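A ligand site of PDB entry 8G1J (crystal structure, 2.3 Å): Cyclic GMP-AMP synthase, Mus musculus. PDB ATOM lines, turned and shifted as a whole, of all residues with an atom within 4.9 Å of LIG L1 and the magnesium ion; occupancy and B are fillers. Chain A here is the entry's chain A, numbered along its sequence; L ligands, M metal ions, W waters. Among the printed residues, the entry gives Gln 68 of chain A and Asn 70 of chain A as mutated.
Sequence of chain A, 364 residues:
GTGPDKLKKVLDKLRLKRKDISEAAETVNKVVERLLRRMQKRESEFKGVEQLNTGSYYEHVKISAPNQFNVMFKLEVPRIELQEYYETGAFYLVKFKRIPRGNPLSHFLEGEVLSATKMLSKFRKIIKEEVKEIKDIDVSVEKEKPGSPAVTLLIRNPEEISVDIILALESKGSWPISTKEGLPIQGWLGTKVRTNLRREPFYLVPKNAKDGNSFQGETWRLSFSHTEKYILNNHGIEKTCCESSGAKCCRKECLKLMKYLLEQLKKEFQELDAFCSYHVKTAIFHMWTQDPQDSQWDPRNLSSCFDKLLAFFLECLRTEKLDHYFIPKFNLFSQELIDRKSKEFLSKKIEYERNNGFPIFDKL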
ATOM      1  N   GLY A  55      19.067  -7.202  20.540  1.00  0.00           N
ATOM      2  CA  GLY A  55      18.571  -6.664  19.291  1.00  0.00           C
ATOM      3  C   GLY A  55      17.522  -5.587  19.482  1.00  0.00           C
ATOM      4  O   GLY A  55      17.181  -5.195  20.607  1.00  0.00           O
ATOM      5  N   SER A  56      16.988  -5.114  18.349  1.00  0.00           N
ATOM      6  CA  SER A  56      16.310  -3.816  18.317  1.00  0.00           C
ATOM      7  C   SER A  56      15.060  -3.793  19.178  1.00  0.00           C
ATOM      8  O   SER A  56      14.739  -2.745  19.757  1.00  0.00           O
ATOM      9  CB  SER A  56      15.928  -3.423  16.876  1.00  0.00           C
ATOM     10  OG  SER A  56      14.992  -4.325  16.296  1.00  0.00           O
ATOM     11  N   GLU A  59      16.069  -3.187  22.575  1.00  0.00           N
ATOM     12  CA  GLU A  59      16.695  -1.872  22.707  1.00  0.00           C
ATOM     13  C   GLU A  59      15.690  -0.750  22.487  1.00  0.00           C
ATOM     14  O   GLU A  59      16.058   0.429  22.577  1.00  0.00           O
ATOM     15  CB  GLU A  59      17.865  -1.757  21.723  1.00  0.00           C
ATOM     16  CG  GLU A  59      19.039  -2.736  22.028  1.00  0.00           C
ATOM     17  CD  GLU A  59      19.919  -2.989  20.792  1.00  0.00           C
ATOM     18  OE1 GLU A  59      19.456  -2.681  19.673  1.00  0.00           O
ATOM     19  OE2 GLU A  59      21.077  -3.481  20.944  1.00  0.00           O
ATOM     20  N   LYS A  62      13.128  -1.106  17.554  1.00  0.00           N
ATOM     21  CA  LYS A  62      12.382  -1.786  16.504  1.00  0.00           C
ATOM     22  C   LYS A  62      11.356  -0.837  15.911  1.00  0.00           C
ATOM     23  O   LYS A  62      10.668  -0.123  16.631  1.00  0.00           O
ATOM     24  CB  LYS A  62      11.662  -3.015  17.094  1.00  0.00           C
ATOM     25  CG  LYS A  62      10.862  -3.831  16.074  1.00  0.00           C
ATOM     26  CD  LYS A  62      11.808  -4.770  15.334  1.00  0.00           C
ATOM     27  CE  LYS A  62      11.115  -5.492  14.166  1.00  0.00           C
ATOM     28  NZ  LYS A  62      10.600  -4.519  13.158  1.00  0.00           N
ATOM     29  N   GLN A  68      10.115  -9.083  14.499  1.00  0.00           N
ATOM     30  CA  GLN A  68      11.436  -9.715  14.445  1.00  0.00           C
ATOM     31  C   GLN A  68      12.072  -9.590  15.811  1.00  0.00           C
ATOM     32  O   GLN A  68      12.369  -8.472  16.237  1.00  0.00           O
ATOM     33  CB  GLN A  68      12.332  -9.098  13.362  1.00  0.00           C
ATOM     34  CG  GLN A  68      13.393 -10.071  12.864  1.00  0.00           C
ATOM     35  CD  GLN A  68      14.754  -9.868  13.501  1.00  0.00           C
ATOM     36  OE1 GLN A  68      14.916  -9.099  14.465  1.00  0.00           O
ATOM     37  NE2 GLN A  68      15.761 -10.548  12.958  1.00  0.00           N
ATOM     38  N   ASN A  70      15.115 -11.098  18.601  1.00  0.00           N
ATOM     39  CA  ASN A  70      16.446 -11.703  18.658  1.00  0.00           C
ATOM     40  C   ASN A  70      16.692 -12.222  20.064  1.00  0.00           C
ATOM     41  O   ASN A  70      16.563 -11.465  21.036  1.00  0.00           O
ATOM     42  CB  ASN A  70      17.525 -10.694  18.279  1.00  0.00           C
ATOM     43  CG  ASN A  70      17.293 -10.088  16.908  1.00  0.00           C
ATOM     44  OD1 ASN A  70      16.828  -8.952  16.793  1.00  0.00           O
ATOM     45  ND2 ASN A  70      17.599 -10.859  15.850  1.00  0.00           N
ATOM     46  N   ARG A 221      32.253 -16.532  15.561  1.00  0.00           N
ATOM     47  CA  ARG A 221      32.305 -15.079  15.418  1.00  0.00           C
ATOM     48  C   ARG A 221      31.964 -14.404  16.746  1.00  0.00           C
ATOM     49  O   ARG A 221      30.999 -14.802  17.420  1.00  0.00           O
ATOM     50  CB  ARG A 221      31.323 -14.550  14.321  1.00  0.00           C
ATOM     51  CG  ARG A 221      31.412 -13.006  14.135  1.00  0.00           C
ATOM     52  CD  ARG A 221      30.508 -12.461  13.033  1.00  0.00           C
ATOM     53  NE  ARG A 221      29.108 -12.510  13.436  1.00  0.00           N
ATOM     54  CZ  ARG A 221      28.075 -12.263  12.622  1.00  0.00           C
ATOM     55  NH1 ARG A 221      28.262 -11.951  11.347  1.00  0.00           N
ATOM     56  NH2 ARG A 221      26.842 -12.341  13.103  1.00  0.00           N
ATOM     57  N   LEU A 222      32.727 -13.367  17.091  1.00  0.00           N
ATOM     58  CA  LEU A 222      32.460 -12.623  18.320  1.00  0.00           C
ATOM     59  C   LEU A 222      31.112 -11.916  18.253  1.00  0.00           C
ATOM     60  O   LEU A 222      30.722 -11.395  17.204  1.00  0.00           O
ATOM     61  CB  LEU A 222      33.536 -11.580  18.583  1.00  0.00           C
ATOM     62  CG  LEU A 222      34.845 -12.132  19.089  1.00  0.00           C
ATOM     63  CD1 LEU A 222      35.900 -11.046  19.023  1.00  0.00           C
ATOM     64  CD2 LEU A 222      34.638 -12.635  20.515  1.00  0.00           C
ATOM     65  N   SER A 225      26.268  -8.343  21.566  1.00  0.00           N
ATOM     66  CA  SER A 225      24.887  -7.894  21.606  1.00  0.00           C
ATOM     67  C   SER A 225      24.498  -7.411  22.990  1.00  0.00           C
ATOM     68  O   SER A 225      23.691  -6.492  23.109  1.00  0.00           O
ATOM     69  CB  SER A 225      23.951  -9.019  21.179  1.00  0.00           C
ATOM     70  OG  SER A 225      24.231  -9.344  19.848  1.00  0.00           O
ATOM     71  N   GLU A 228      26.046  -3.911  23.339  1.00  0.00           N
ATOM     72  CA  GLU A 228      25.288  -2.960  22.526  1.00  0.00           C
ATOM     73  C   GLU A 228      23.953  -2.616  23.177  1.00  0.00           C
ATOM     74  O   GLU A 228      23.532  -1.446  23.160  1.00  0.00           O
ATOM     75  CB  GLU A 228      25.076  -3.546  21.141  1.00  0.00           C
ATOM     76  CG  GLU A 228      26.387  -3.887  20.438  1.00  0.00           C
ATOM     77  CD  GLU A 228      26.174  -4.710  19.196  1.00  0.00           C
ATOM     78  OE1 GLU A 228      24.987  -4.860  18.781  1.00  0.00           O
ATOM     79  OE2 GLU A 228      27.183  -5.175  18.630  1.00  0.00           O
ATOM     80  N   LYS A 259      17.504   3.286  10.175  1.00  0.00           N
ATOM     81  CA  LYS A 259      17.062   1.903   9.982  1.00  0.00           C
ATOM     82  C   LYS A 259      15.949   1.850   8.941  1.00  0.00           C
ATOM     83  O   LYS A 259      15.978   0.994   8.043  1.00  0.00           O
ATOM     84  CB  LYS A 259      16.553   1.319  11.305  1.00  0.00           C
ATOM     85  CG  LYS A 259      17.660   0.990  12.314  1.00  0.00           C
ATOM     86  CD  LYS A 259      17.104   0.767  13.726  1.00  0.00           C
ATOM     87  CE  LYS A 259      16.113  -0.408  13.757  1.00  0.00           C
ATOM     88  NZ  LYS A 259      16.737  -1.712  13.435  1.00  0.00           N
ATOM     89  N   GLU A 263      15.740  -0.080   5.417  1.00  0.00           N
ATOM     90  CA  GLU A 263      14.691  -1.099   5.226  1.00  0.00           C
ATOM     91  C   GLU A 263      13.830  -0.798   4.002  1.00  0.00           C
ATOM     92  O   GLU A 263      13.552  -1.701   3.192  1.00  0.00           O
ATOM     93  CB  GLU A 263      13.795  -1.213   6.472  1.00  0.00           C
ATOM     94  CG  GLU A 263      14.355  -1.965   7.661  1.00  0.00           C
ATOM     95  CD  GLU A 263      13.327  -2.137   8.796  1.00  0.00           C
ATOM     96  OE1 GLU A 263      12.113  -2.264   8.474  1.00  0.00           O
ATOM     97  OE2 GLU A 263      13.712  -2.115  10.002  1.00  0.00           O
ATOM     98  N   SER A 277      21.035  -3.980   8.851  1.00  0.00           N
ATOM     99  CA  SER A 277      20.858  -2.939   9.841  1.00  0.00           C
ATOM    100  C   SER A 277      22.059  -2.808  10.779  1.00  0.00           C
ATOM    101  O   SER A 277      22.252  -1.737  11.366  1.00  0.00           O
ATOM    102  CB  SER A 277      19.574  -3.188  10.619  1.00  0.00           C
ATOM    103  OG  SER A 277      19.677  -4.372  11.361  1.00  0.00           O
ATOM    104  N   TYR A 278      22.872  -3.852  10.936  1.00  0.00           N
ATOM    105  CA  TYR A 278      24.042  -3.709  11.813  1.00  0.00           C
ATOM    106  C   TYR A 278      25.011  -2.662  11.265  1.00  0.00           C
ATOM    107  O   TYR A 278      25.736  -2.005  12.039  1.00  0.00           O
ATOM    108  CB  TYR A 278      24.756  -5.061  11.996  1.00  0.00           C
ATOM    109  CG  TYR A 278      25.775  -5.055  13.137  1.00  0.00           C
ATOM    110  CD1 TYR A 278      25.366  -4.882  14.450  1.00  0.00           C
ATOM    111  CD2 TYR A 278      27.141  -5.196  12.885  1.00  0.00           C
ATOM    112  CE1 TYR A 278      26.263  -4.870  15.479  1.00  0.00           C
ATOM    113  CE2 TYR A 278      28.060  -5.183  13.919  1.00  0.00           C
ATOM    114  CZ  TYR A 278      27.607  -5.012  15.222  1.00  0.00           C
ATOM    115  OH  TYR A 278      28.465  -4.999  16.284  1.00  0.00           O
ATOM    116  N   LYS A 281      23.688   0.462  12.712  1.00  0.00           N
ATOM    117  CA  LYS A 281      23.922   0.519  14.159  1.00  0.00           C
ATOM    118  C   LYS A 281      25.392   0.825  14.464  1.00  0.00           C
ATOM    119  O   LYS A 281      25.693   1.630  15.359  1.00  0.00           O
ATOM    120  CB  LYS A 281      23.491  -0.812  14.781  1.00  0.00           C
ATOM    121  CG  LYS A 281      23.546  -0.937  16.331  1.00  0.00           C
ATOM    122  CD  LYS A 281      22.959  -2.293  16.780  1.00  0.00           C
ATOM    123  CE  LYS A 281      22.667  -2.347  18.297  1.00  0.00           C
ATOM    124  NZ  LYS A 281      22.418  -3.745  18.829  1.00  0.00           N
ATOM    125  N   HIS A 324      34.175  -2.116  12.515  1.00  0.00           N
ATOM    126  CA  HIS A 324      33.481  -2.706  13.631  1.00  0.00           C
ATOM    127  C   HIS A 324      33.759  -1.879  14.888  1.00  0.00           C
ATOM    128  O   HIS A 324      34.917  -1.524  15.159  1.00  0.00           O
ATOM    129  CB  HIS A 324      33.929  -4.165  13.822  1.00  0.00           C
ATOM    130  CG  HIS A 324      32.976  -4.967  14.644  1.00  0.00           C
ATOM    131  ND1 HIS A 324      32.805  -4.775  15.997  1.00  0.00           N
ATOM    132  CD2 HIS A 324      32.123  -5.969  14.302  1.00  0.00           C
ATOM    133  CE1 HIS A 324      31.896  -5.622  16.455  1.00  0.00           C
ATOM    134  NE2 HIS A 324      31.476  -6.360  15.442  1.00  0.00           N
HETATM  135  P1  LIG L   1      16.410  -5.082  13.204  1.00  0.00           P
HETATM  136  O1  LIG L   1      16.854  -4.983  11.793  1.00  0.00           O
HETATM  137  O2  LIG L   1      15.315  -4.088  13.607  1.00  0.00           O
HETATM  138  O3  LIG L   1      15.981  -6.489  13.605  1.00  0.00           O
HETATM  139  P2  LIG L   1      18.655  -5.601  15.073  1.00  0.00           P
HETATM  140  O4  LIG L   1      19.714  -4.768  15.734  1.00  0.00           O
HETATM  141  O5  LIG L   1      17.822  -6.467  16.027  1.00  0.00           O
HETATM  142  O6  LIG L   1      17.644  -4.779  14.177  1.00  0.00           O
HETATM  143  P3  LIG L   1      19.344  -8.124  13.698  1.00  0.00           P
HETATM  144  O7  LIG L   1      19.751  -8.341  12.288  1.00  0.00           O
HETATM  145  O8  LIG L   1      17.999  -8.669  14.112  1.00  0.00           O
HETATM  146  O9  LIG L   1      19.290  -6.562  13.977  1.00  0.00           O
HETATM  147  O10 LIG L   1      20.546  -8.646  14.586  1.00  0.00           O
HETATM  148  C1  LIG L   1      20.428  -8.798  16.017  1.00  0.00           C
HETATM  149  C2  LIG L   1      21.717  -8.404  16.713  1.00  0.00           C
HETATM  150  O11 LIG L   1      22.790  -9.292  16.334  1.00  0.00           O
HETATM  151  C3  LIG L   1      22.253  -7.006  16.411  1.00  0.00           C
HETATM  152  O12 LIG L   1      21.612  -6.021  17.214  1.00  0.00           O
HETATM  153  C4  LIG L   1      23.749  -7.151  16.698  1.00  0.00           C
HETATM  154  O13 LIG L   1      24.102  -7.017  18.071  1.00  0.00           O
HETATM  155  C5  LIG L   1      24.025  -8.601  16.270  1.00  0.00           C
HETATM  156  N1  LIG L   1      24.534  -8.699  14.907  1.00  0.00           N
HETATM  157  C6  LIG L   1      23.783  -8.717  13.747  1.00  0.00           C
HETATM  158  N2  LIG L   1      24.511  -8.779  12.652  1.00  0.00           N
HETATM  159  C7  LIG L   1      25.809  -8.752  13.115  1.00  0.00           C
HETATM  160  C8  LIG L   1      27.059  -8.790  12.455  1.00  0.00           C
HETATM  161  N3  LIG L   1      27.195  -8.858  11.121  1.00  0.00           N
HETATM  162  N4  LIG L   1      28.171  -8.771  13.215  1.00  0.00           N
HETATM  163  C9  LIG L   1      28.056  -8.716  14.543  1.00  0.00           C
HETATM  164  N5  LIG L   1      26.932  -8.668  15.271  1.00  0.00           N
HETATM  165  C10 LIG L   1      25.846  -8.702  14.500  1.00  0.00           C
HETATM  166  P1  LG2 L   2      25.748 -12.159   6.388  1.00  0.00           P
HETATM  167  O1  LG2 L   2      24.483 -11.355   6.723  1.00  0.00           O
HETATM  168  O2  LG2 L   2      27.024 -11.426   6.779  1.00  0.00           O
HETATM  169  O3  LG2 L   2      25.727 -12.467   4.904  1.00  0.00           O
HETATM  170  O4  LG2 L   2      25.795 -13.555   7.186  1.00  0.00           O
HETATM  171  P2  LG2 L   2      24.467 -14.330   7.701  1.00  0.00           P
HETATM  172  O5  LG2 L   2      23.207 -13.770   7.068  1.00  0.00           O
HETATM  173  O6  LG2 L   2      24.622 -15.823   7.502  1.00  0.00           O
HETATM  174  O7  LG2 L   2      24.547 -13.952   9.268  1.00  0.00           O
HETATM  175  P3  LG2 L   2      24.027 -12.571   9.907  1.00  0.00           P
HETATM  176  O8  LG2 L   2      25.241 -11.811  10.399  1.00  0.00           O
HETATM  177  O9  LG2 L   2      23.135 -11.757   8.995  1.00  0.00           O
HETATM  178  O10 LG2 L   2      23.164 -13.159  11.135  1.00  0.00           O
HETATM  179  C1  LG2 L   2      21.910 -13.745  10.863  1.00  0.00           C
HETATM  180  C2  LG2 L   2      20.907 -13.253  11.900  1.00  0.00           C
HETATM  181  O11 LG2 L   2      21.212 -13.900  13.128  1.00  0.00           O
HETATM  182  C3  LG2 L   2      20.993 -11.754  12.189  1.00  0.00           C
HETATM  183  O12 LG2 L   2      20.168 -10.979  11.352  1.00  0.00           O
HETATM  184  C4  LG2 L   2      20.537 -11.714  13.635  1.00  0.00           C
HETATM  185  O13 LG2 L   2      19.119 -11.735  13.662  1.00  0.00           O
HETATM  186  C5  LG2 L   2      21.078 -13.003  14.225  1.00  0.00           C
HETATM  187  N1  LG2 L   2      22.404 -12.711  14.810  1.00  0.00           N
HETATM  188  C6  LG2 L   2      23.609 -12.775  14.133  1.00  0.00           C
HETATM  189  N2  LG2 L   2      24.609 -12.452  14.999  1.00  0.00           N
HETATM  190  C7  LG2 L   2      24.070 -12.192  16.219  1.00  0.00           C
HETATM  191  C8  LG2 L   2      24.630 -11.787  17.441  1.00  0.00           C
HETATM  192  O14 LG2 L   2      25.838 -11.628  17.550  1.00  0.00           O
HETATM  193  N3  LG2 L   2      23.810 -11.584  18.539  1.00  0.00           N
HETATM  194  C9  LG2 L   2      22.446 -11.741  18.428  1.00  0.00           C
HETATM  195  N4  LG2 L   2      21.893 -12.125  17.206  1.00  0.00           N
HETATM  196  C10 LG2 L   2      22.685 -12.345  16.116  1.00  0.00           C
HETATM  197 MG    MG M   1      16.380  -7.734  15.070  1.00  0.00          MG
HETATM  198  O   HOH W   1      19.337  -2.541  17.012  1.00  0.00           O
HETATM  199  O   HOH W   2      27.676  -7.678  18.175  1.00  0.00           O
HETATM  200  O   HOH W   3      14.698  -7.077  16.410  1.00  0.00           O
HETATM  201  O   HOH W   4      21.608  -6.375  10.732  1.00  0.00           O
HETATM  202  O   HOH W   5      21.343  -3.659  13.746  1.00  0.00           O
HETATM  203  O   HOH W   6      13.067  -2.978  12.787  1.00  0.00           O
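The side-chain carboxylate of Glu 228 lies within hydrogen-bond range of an oxygen (O13) of LIG L1, at 2.4 Å.
The side-chain hydroxyl of Ser 225 lies within hydrogen-bond range of a nitrogen (N3) of LG2 L2 (2.6 Å).
O5 of LIG L1 lies close to N of Ser 56.
O13 of LIG L1 is in hydrogen-bond range of OG of Ser 225.
The side-chain hydroxyl (OG) of Ser 277 lies within hydrogen-bond range of an oxygen (O1) of LIG L1.
O2 of LIG L1 sits at hydrogen-bond distance from OG of Ser 56 (2.7 Å).
ND2 of Asn 70 sits at hydrogen-bond distance from O13 of LG2 L2 (2.8 Å).
The side-chain amino group (NZ) of Lys 281 is in hydrogen-bond range of an oxygen (O12) of LIG L1 (2.9 Å).
NH1 of Arg 221 lies within salt-bridge range of O8 of LG2 L2 (3.2 Å).
NZ of Lys 259 lies within salt-bridge range of O2 of LIG L1 (2.8 Å).
An oxygen (O7) of LIG L1 sits at hydrogen-bond distance from an oxygen (O12) of LG2 L2 (2.8 Å).
The side-chain amino group (NZ) of Lys 281 is in salt-bridge range of the side-chain carboxylate (OE2) of Glu 59 (2.5 Å).
The side-chain hydroxyl (OH) of Tyr 278 sits at hydrogen-bond distance from a ring nitrogen (NE2) of His 324, at 3.4 Å.
The side-chain carboxylate (OE1) of Glu 228 lies within salt-bridge range of the side-chain amino group (NZ) of Lys 281, at 2.8 Å.
The backbone NH (N) of Lys 62 lies within hydrogen-bond range of the backbone carbonyl oxygen (O) of Ser 56 (3.2 Å).
The side-chain hydroxyl (OH) of Tyr 278 sits at hydrogen-bond distance from the side-chain carboxylate (OE2) of Glu 228, 2.7 Å away.
The guanidinium group (NH1) of Arg 221 lies close to a nitrogen (N3) of LIG L1.
Residues that only touch LIG L1: Gly 55, Lys 62 and Tyr 278.
Ser 56 touches the magnesium ion.
Three residues have an atom within 4 Å of the magnesium ion: Ser 56, Gln 68 and Asn 70.
The nearest printed residue that does not touch the magnesium ion is Gly 55 (4.9 Å).
O3 of LIG L1 is bound to the magnesium ion.
OE1 of Gln 68 binds the magnesium ion (2.1 Å).
The magnesium ion is bound by O8 of LIG L1 (2.1 Å).
O5 of LIG L1 is bound to the magnesium ion.
OD1 of Asn 70 binds the magnesium ion, 2.2 Å away.
Water W3 is bound to the magnesium ion (2.2 Å).
Water W3 bridges O of Gln 68 (2.7 Å) and OG of Ser 56 (2.8 Å).
Water W1 lies within hydrogen-bond range of an oxygen (O4) of LIG L1 (2.6 Å) and the side-chain carboxylate of Glu 59 (2.7 Å).
Water W6 lies within hydrogen-bond range of an oxygen (O2) of LIG L1, the side-chain amino group (NZ) of Lys 62 and the side-chain carboxylate (OE2) of Glu 263.
Water W5 lies within hydrogen-bond range of O4 of LIG L1 (2.8 Å), OG of Ser 277 (3.0 Å) and N of Tyr 278 (3.2 Å).
Water W4 lies within hydrogen-bond range of the backbone NH (N) of Tyr 278 (2.8 Å), the side-chain hydroxyl (OG) of Ser 277 (2.9 Å) and an oxygen (O7) of LIG L1 (3.1 Å).
Water W2 lies within hydrogen-bond range of OE2 of Glu 228 (2.6 Å), N5 of LIG L1 (3.2 Å) and OH of Tyr 278 (3.4 Å).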
